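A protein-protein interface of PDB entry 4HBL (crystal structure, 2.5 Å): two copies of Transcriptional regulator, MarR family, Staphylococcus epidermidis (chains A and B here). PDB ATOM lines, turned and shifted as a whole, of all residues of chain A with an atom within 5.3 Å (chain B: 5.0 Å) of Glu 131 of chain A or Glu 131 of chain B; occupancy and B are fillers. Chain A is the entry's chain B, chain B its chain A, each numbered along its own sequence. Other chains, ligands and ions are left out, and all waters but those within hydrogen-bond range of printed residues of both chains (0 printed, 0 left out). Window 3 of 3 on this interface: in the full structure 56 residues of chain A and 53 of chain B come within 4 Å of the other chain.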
ATOM      1  N   THR A 126     -11.440  -2.436 -40.270  1.00  0.00           N
ATOM      2  CA  THR A 126     -10.233  -3.060 -39.744  1.00  0.00           C
ATOM      3  C   THR A 126     -10.422  -3.611 -38.330  1.00  0.00           C
ATOM      4  O   THR A 126     -10.215  -4.804 -38.115  1.00  0.00           O
ATOM      5  CB  THR A 126      -9.047  -2.083 -39.715  1.00  0.00           C
ATOM      6  OG1 THR A 126      -8.975  -1.399 -40.961  1.00  0.00           O
ATOM      7  CG2 THR A 126      -7.738  -2.828 -39.474  1.00  0.00           C
ATOM      8  N   THR A 127     -10.844  -2.756 -37.391  1.00  0.00           N
ATOM      9  CA  THR A 127     -10.773  -3.075 -35.953  1.00  0.00           C
ATOM     10  C   THR A 127     -11.726  -4.177 -35.437  1.00  0.00           C
ATOM     11  O   THR A 127     -11.314  -5.005 -34.602  1.00  0.00           O
ATOM     12  CB  THR A 127     -10.828  -1.819 -35.043  1.00  0.00           C
ATOM     13  OG1 THR A 127     -12.077  -1.138 -35.216  1.00  0.00           O
ATOM     14  CG2 THR A 127      -9.667  -0.867 -35.343  1.00  0.00           C
ATOM     15  N   GLU A 128     -12.970  -4.223 -35.922  1.00  0.00           N
ATOM     16  CA  GLU A 128     -13.871  -5.324 -35.534  1.00  0.00           C
ATOM     17  C   GLU A 128     -13.291  -6.647 -36.038  1.00  0.00           C
ATOM     18  O   GLU A 128     -13.444  -7.693 -35.406  1.00  0.00           O
ATOM     19  CB  GLU A 128     -15.292  -5.094 -36.070  1.00  0.00           C
ATOM     20  CG  GLU A 128     -16.400  -5.945 -35.439  1.00  0.00           C
ATOM     21  CD  GLU A 128     -17.776  -5.763 -36.103  1.00  0.00           C
ATOM     22  OE1 GLU A 128     -18.076  -4.667 -36.627  1.00  0.00           O
ATOM     23  OE2 GLU A 128     -18.581  -6.719 -36.087  1.00  0.00           O
ATOM     24  N   TYR A 129     -12.617  -6.577 -37.184  1.00  0.00           N
ATOM     25  CA  TYR A 129     -11.958  -7.729 -37.786  1.00  0.00           C
ATOM     26  C   TYR A 129     -10.736  -8.139 -36.957  1.00  0.00           C
ATOM     27  O   TYR A 129     -10.553  -9.313 -36.663  1.00  0.00           O
ATOM     28  CB  TYR A 129     -11.525  -7.413 -39.220  1.00  0.00           C
ATOM     29  CG  TYR A 129     -12.535  -7.693 -40.316  1.00  0.00           C
ATOM     30  CD1 TYR A 129     -13.549  -6.774 -40.602  1.00  0.00           C
ATOM     31  CD2 TYR A 129     -12.449  -8.854 -41.103  1.00  0.00           C
ATOM     32  CE1 TYR A 129     -14.462  -7.009 -41.618  1.00  0.00           C
ATOM     33  CE2 TYR A 129     -13.363  -9.094 -42.116  1.00  0.00           C
ATOM     34  CZ  TYR A 129     -14.369  -8.165 -42.377  1.00  0.00           C
ATOM     35  OH  TYR A 129     -15.298  -8.369 -43.389  1.00  0.00           O
ATOM     36  N   ASP A 130      -9.896  -7.166 -36.598  1.00  0.00           N
ATOM     37  CA  ASP A 130      -8.726  -7.414 -35.730  1.00  0.00           C
ATOM     38  C   ASP A 130      -9.074  -8.046 -34.381  1.00  0.00           C
ATOM     39  O   ASP A 130      -8.317  -8.865 -33.896  1.00  0.00           O
ATOM     40  CB  ASP A 130      -7.897  -6.147 -35.466  1.00  0.00           C
ATOM     41  CG  ASP A 130      -6.583  -6.454 -34.724  1.00  0.00           C
ATOM     42  OD1 ASP A 130      -5.631  -6.918 -35.374  1.00  0.00           O
ATOM     43  OD2 ASP A 130      -6.498  -6.272 -33.488  1.00  0.00           O
ATOM     44  N   GLU A 131     -10.224  -7.685 -33.809  1.00  0.00           N
ATOM     45  CA  GLU A 131     -10.671  -8.248 -32.528  1.00  0.00           C
ATOM     46  C   GLU A 131     -11.010  -9.729 -32.648  1.00  0.00           C
ATOM     47  O   GLU A 131     -10.580 -10.541 -31.841  1.00  0.00           O
ATOM     48  CB  GLU A 131     -11.894  -7.501 -32.040  1.00  0.00           C
ATOM     49  CG  GLU A 131     -12.119  -7.595 -30.546  1.00  0.00           C
ATOM     50  CD  GLU A 131     -13.357  -6.830 -30.122  1.00  0.00           C
ATOM     51  OE1 GLU A 131     -14.148  -7.408 -29.355  1.00  0.00           O
ATOM     52  OE2 GLU A 131     -13.551  -5.658 -30.561  1.00  0.00           O
ATOM     53  N   THR A 132     -11.800 -10.050 -33.665  1.00  0.00           N
ATOM     54  CA  THR A 132     -12.219 -11.405 -33.958  1.00  0.00           C
ATOM     55  C   THR A 132     -11.016 -12.304 -34.372  1.00  0.00           C
ATOM     56  O   THR A 132     -10.841 -13.405 -33.863  1.00  0.00           O
ATOM     57  CB  THR A 132     -13.270 -11.349 -35.065  1.00  0.00           C
ATOM     58  OG1 THR A 132     -12.828 -10.402 -36.034  1.00  0.00           O
ATOM     59  CG2 THR A 132     -14.615 -10.832 -34.537  1.00  0.00           C
ATOM     60  N   LYS A 133     -10.195 -11.827 -35.306  1.00  0.00           N
ATOM     61  CA  LYS A 133      -8.921 -12.490 -35.662  1.00  0.00           C
ATOM     62  C   LYS A 133      -8.119 -12.852 -34.402  1.00  0.00           C
ATOM     63  O   LYS A 133      -7.669 -13.974 -34.247  1.00  0.00           O
ATOM     64  CB  LYS A 133      -8.109 -11.547 -36.560  1.00  0.00           C
ATOM     65  CG  LYS A 133      -7.213 -12.205 -37.580  1.00  0.00           C
ATOM     66  CD  LYS A 133      -7.012 -11.293 -38.793  1.00  0.00           C
ATOM     67  CE  LYS A 133      -5.743 -10.433 -38.712  1.00  0.00           C
ATOM     68  NZ  LYS A 133      -4.485 -11.184 -38.377  1.00  0.00           N
ATOM     69  N   TYR A 134      -7.981 -11.882 -33.498  1.00  0.00           N
ATOM     70  CA  TYR A 134      -7.303 -12.052 -32.201  1.00  0.00           C
ATOM     71  C   TYR A 134      -7.801 -13.204 -31.342  1.00  0.00           C
ATOM     72  O   TYR A 134      -6.993 -13.977 -30.788  1.00  0.00           O
ATOM     73  CB  TYR A 134      -7.378 -10.751 -31.379  1.00  0.00           C
ATOM     74  CG  TYR A 134      -6.780 -10.833 -29.975  1.00  0.00           C
ATOM     75  CD1 TYR A 134      -5.420 -11.181 -29.779  1.00  0.00           C
ATOM     76  CD2 TYR A 134      -7.578 -10.578 -28.846  1.00  0.00           C
ATOM     77  CE1 TYR A 134      -4.877 -11.286 -28.506  1.00  0.00           C
ATOM     78  CE2 TYR A 134      -7.044 -10.675 -27.577  1.00  0.00           C
ATOM     79  CZ  TYR A 134      -5.693 -11.032 -27.399  1.00  0.00           C
ATOM     80  OH  TYR A 134      -5.164 -11.050 -26.104  1.00  0.00           O
ATOM     81  N   VAL A 135      -9.124 -13.265 -31.200  1.00  0.00           N
ATOM     82  CA  VAL A 135      -9.783 -14.317 -30.433  1.00  0.00           C
ATOM     83  C   VAL A 135      -9.498 -15.671 -31.061  1.00  0.00           C
ATOM     84  O   VAL A 135      -9.099 -16.572 -30.347  1.00  0.00           O
ATOM     85  CB  VAL A 135     -11.301 -14.044 -30.309  1.00  0.00           C
ATOM     86  CG1 VAL A 135     -12.075 -15.290 -29.841  1.00  0.00           C
ATOM     87  CG2 VAL A 135     -11.529 -12.813 -29.447  1.00  0.00           C
ATOM     88  N   THR B 126     -12.442 -13.169 -16.977  1.00  0.00           N
ATOM     89  CA  THR B 126     -13.855 -13.324 -17.318  1.00  0.00           C
ATOM     90  C   THR B 126     -14.353 -12.269 -18.274  1.00  0.00           C
ATOM     91  O   THR B 126     -15.304 -12.491 -18.997  1.00  0.00           O
ATOM     92  CB  THR B 126     -14.816 -13.475 -16.115  1.00  0.00           C
ATOM     93  OG1 THR B 126     -14.511 -12.518 -15.131  1.00  0.00           O
ATOM     94  CG2 THR B 126     -14.661 -14.826 -15.504  1.00  0.00           C
ATOM     95  N   THR B 127     -13.706 -11.128 -18.286  1.00  0.00           N
ATOM     96  CA  THR B 127     -14.143 -10.061 -19.159  1.00  0.00           C
ATOM     97  C   THR B 127     -13.809 -10.442 -20.588  1.00  0.00           C
ATOM     98  O   THR B 127     -14.599 -10.231 -21.500  1.00  0.00           O
ATOM     99  CB  THR B 127     -13.464  -8.743 -18.777  1.00  0.00           C
ATOM    100  OG1 THR B 127     -13.762  -8.477 -17.407  1.00  0.00           O
ATOM    101  CG2 THR B 127     -13.989  -7.575 -19.623  1.00  0.00           C
ATOM    102  N   GLU B 128     -12.639 -11.037 -20.765  1.00  0.00           N
ATOM    103  CA  GLU B 128     -12.212 -11.431 -22.061  1.00  0.00           C
ATOM    104  C   GLU B 128     -12.926 -12.711 -22.521  1.00  0.00           C
ATOM    105  O   GLU B 128     -13.062 -12.944 -23.727  1.00  0.00           O
ATOM    106  CB  GLU B 128     -10.691 -11.565 -22.094  1.00  0.00           C
ATOM    107  CG  GLU B 128     -10.068 -11.451 -23.487  1.00  0.00           C
ATOM    108  CD  GLU B 128     -10.355 -10.119 -24.170  1.00  0.00           C
ATOM    109  OE1 GLU B 128     -10.667  -9.133 -23.458  1.00  0.00           O
ATOM    110  OE2 GLU B 128     -10.260 -10.046 -25.424  1.00  0.00           O
ATOM    111  N   TYR B 129     -13.377 -13.525 -21.561  1.00  0.00           N
ATOM    112  CA  TYR B 129     -14.169 -14.714 -21.876  1.00  0.00           C
ATOM    113  C   TYR B 129     -15.549 -14.275 -22.309  1.00  0.00           C
ATOM    114  O   TYR B 129     -16.179 -14.901 -23.144  1.00  0.00           O
ATOM    115  CB  TYR B 129     -14.307 -15.631 -20.693  1.00  0.00           C
ATOM    116  CG  TYR B 129     -13.081 -16.430 -20.336  1.00  0.00           C
ATOM    117  CD1 TYR B 129     -12.187 -16.831 -21.303  1.00  0.00           C
ATOM    118  CD2 TYR B 129     -12.856 -16.845 -19.024  1.00  0.00           C
ATOM    119  CE1 TYR B 129     -11.082 -17.588 -20.989  1.00  0.00           C
ATOM    120  CE2 TYR B 129     -11.747 -17.613 -18.686  1.00  0.00           C
ATOM    121  CZ  TYR B 129     -10.855 -17.966 -19.685  1.00  0.00           C
ATOM    122  OH  TYR B 129      -9.733 -18.723 -19.402  1.00  0.00           O
ATOM    123  N   ASP B 130     -16.027 -13.184 -21.757  1.00  0.00           N
ATOM    124  CA  ASP B 130     -17.272 -12.624 -22.246  1.00  0.00           C
ATOM    125  C   ASP B 130     -17.109 -11.943 -23.582  1.00  0.00           C
ATOM    126  O   ASP B 130     -18.010 -11.977 -24.419  1.00  0.00           O
ATOM    127  CB  ASP B 130     -17.880 -11.690 -21.221  1.00  0.00           C
ATOM    128  CG  ASP B 130     -18.368 -12.435 -20.000  1.00  0.00           C
ATOM    129  OD1 ASP B 130     -18.524 -11.791 -18.943  1.00  0.00           O
ATOM    130  OD2 ASP B 130     -18.597 -13.667 -20.079  1.00  0.00           O
ATOM    131  N   GLU B 131     -15.952 -11.322 -23.760  1.00  0.00           N
ATOM    132  CA  GLU B 131     -15.554 -10.764 -25.036  1.00  0.00           C
ATOM    133  C   GLU B 131     -15.565 -11.831 -26.122  1.00  0.00           C
ATOM    134  O   GLU B 131     -16.053 -11.615 -27.208  1.00  0.00           O
ATOM    135  CB  GLU B 131     -14.133 -10.211 -24.935  1.00  0.00           C
ATOM    136  CG  GLU B 131     -13.714  -9.428 -26.169  1.00  0.00           C
ATOM    137  CD  GLU B 131     -14.518  -8.156 -26.333  1.00  0.00           C
ATOM    138  OE1 GLU B 131     -15.762  -8.206 -26.293  1.00  0.00           O
ATOM    139  OE2 GLU B 131     -13.898  -7.087 -26.491  1.00  0.00           O
ATOM    140  N   THR B 132     -14.999 -12.976 -25.799  1.00  0.00           N
ATOM    141  CA  THR B 132     -14.921 -14.089 -26.694  1.00  0.00           C
ATOM    142  C   THR B 132     -16.304 -14.564 -27.185  1.00  0.00           C
ATOM    143  O   THR B 132     -16.493 -14.742 -28.396  1.00  0.00           O
ATOM    144  CB  THR B 132     -14.142 -15.205 -26.013  1.00  0.00           C
ATOM    145  OG1 THR B 132     -12.821 -14.718 -25.749  1.00  0.00           O
ATOM    146  CG2 THR B 132     -14.046 -16.409 -26.917  1.00  0.00           C
ATOM    147  N   LYS B 133     -17.243 -14.749 -26.250  1.00  0.00           N
ATOM    148  CA  LYS B 133     -18.611 -15.161 -26.546  1.00  0.00           C
ATOM    149  C   LYS B 133     -19.328 -14.156 -27.423  1.00  0.00           C
ATOM    150  O   LYS B 133     -20.002 -14.547 -28.368  1.00  0.00           O
ATOM    151  CB  LYS B 133     -19.420 -15.338 -25.253  1.00  0.00           C
ATOM    152  CG  LYS B 133     -19.463 -16.731 -24.635  1.00  0.00           C
ATOM    153  CD  LYS B 133     -19.355 -16.634 -23.110  1.00  0.00           C
ATOM    154  CE  LYS B 133     -20.596 -16.075 -22.413  1.00  0.00           C
ATOM    155  NZ  LYS B 133     -21.711 -17.080 -22.383  1.00  0.00           N
ATOM    156  N   TYR B 134     -19.210 -12.872 -27.086  1.00  0.00           N
ATOM    157  CA  TYR B 134     -19.762 -11.778 -27.888  1.00  0.00           C
ATOM    158  C   TYR B 134     -19.205 -11.819 -29.318  1.00  0.00           C
ATOM    159  O   TYR B 134     -19.922 -11.565 -30.277  1.00  0.00           O
ATOM    160  CB  TYR B 134     -19.409 -10.434 -27.230  1.00  0.00           C
ATOM    161  CG  TYR B 134     -19.992  -9.162 -27.849  1.00  0.00           C
ATOM    162  CD1 TYR B 134     -21.245  -8.695 -27.452  1.00  0.00           C
ATOM    163  CD2 TYR B 134     -19.266  -8.379 -28.791  1.00  0.00           C
ATOM    164  CE1 TYR B 134     -21.775  -7.506 -27.968  1.00  0.00           C
ATOM    165  CE2 TYR B 134     -19.802  -7.194 -29.336  1.00  0.00           C
ATOM    166  CZ  TYR B 134     -21.061  -6.760 -28.910  1.00  0.00           C
ATOM    167  OH  TYR B 134     -21.653  -5.592 -29.377  1.00  0.00           O
ATOM    168  N   VAL B 135     -17.917 -12.128 -29.453  1.00  0.00           N
ATOM    169  CA  VAL B 135     -17.255 -12.067 -30.746  1.00  0.00           C
ATOM    170  C   VAL B 135     -17.786 -13.181 -31.627  1.00  0.00           C
ATOM    171  O   VAL B 135     -18.073 -12.947 -32.812  1.00  0.00           O
ATOM    172  CB  VAL B 135     -15.718 -12.144 -30.595  1.00  0.00           C
ATOM    173  CG1 VAL B 135     -15.046 -12.858 -31.777  1.00  0.00           C
ATOM    174  CG2 VAL B 135     -15.146 -10.742 -30.415  1.00  0.00           C
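Among the printed residues, pairs that only touch across the chains: Glu 131 of chain A with Val 135 of chain B, Thr 132 of chain A with Val 135 of chain B, Tyr 134 of chain A with Glu 128 of chain B and Val 135 of chain A with Thr 132 of chain B.
Of chain B, only Glu 131 and Val 135 come within 4 Å of Glu 131 of chain A. Glu 131 of chain B touches just one residue of chain A: Glu 131 (2.9 Å). Printed residues of chain A within 4 Å of Glu 128 of chain B: Tyr 134. Of the printed residues of chain B, Tyr 134 of chain A touches Glu 128 (3.9 Å). Of the printed residues of chain A, Thr 132 of chain B touches Val 135 (3.7 Å). Thr 126 of chain B touches none of the printed residues of chain A. The nearest printed residue of chain B that does not touch Glu 131 of chain A is Tyr 134 of chain B (5.2 Å). The nearest printed residue of chain B that does not touch Tyr 134 of chain A is Glu 131 of chain B (6.8 Å).
Hydrophobic or aromatic side chains of chain B within 4 Å of the printed part of chain A: Val 135. Among the printed residues, no Asp or Glu carboxylate lies within 4 Å of a Lys or Arg side-chain nitrogen of the other chain.
OE2 of Glu 131 of chain B sits close to OE1 of Glu 131 of chain A.
The side-chain hydroxyl (OG1) of Thr 132 of chain B is in hydrogen-bond range of the backbone carbonyl oxygen (O) of Glu 128 of chain B, 2.7 Å away. The backbone carbonyl oxygen of Glu 128 of chain A sits at hydrogen-bond distance from the side-chain hydroxyl of Thr 132 of chain A (2.8 Å). O of Tyr 129 of chain A lies within hydrogen-bond range of OG1 of Thr 132 of chain A, 2.6 Å away.
Glu 131 of chain A touches its own counterpart, Glu 131 of chain B. Glu 131 of chain A touches Val 135 of chain B, but with the chains exchanged Val 135 of chain A does not touch Glu 131 of chain B (5.2 Å). Thr 132 of chain A touches Val 135 of chain B, and with the chains exchanged Val 135 of chain A touches Thr 132 of chain B. Tyr 134 of chain A touches Glu 128 of chain B, but with the chains exchanged Glu 128 of chain A does not touch Tyr 134 of chain B (6.9 Å). 10 positions are printed for both chains.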
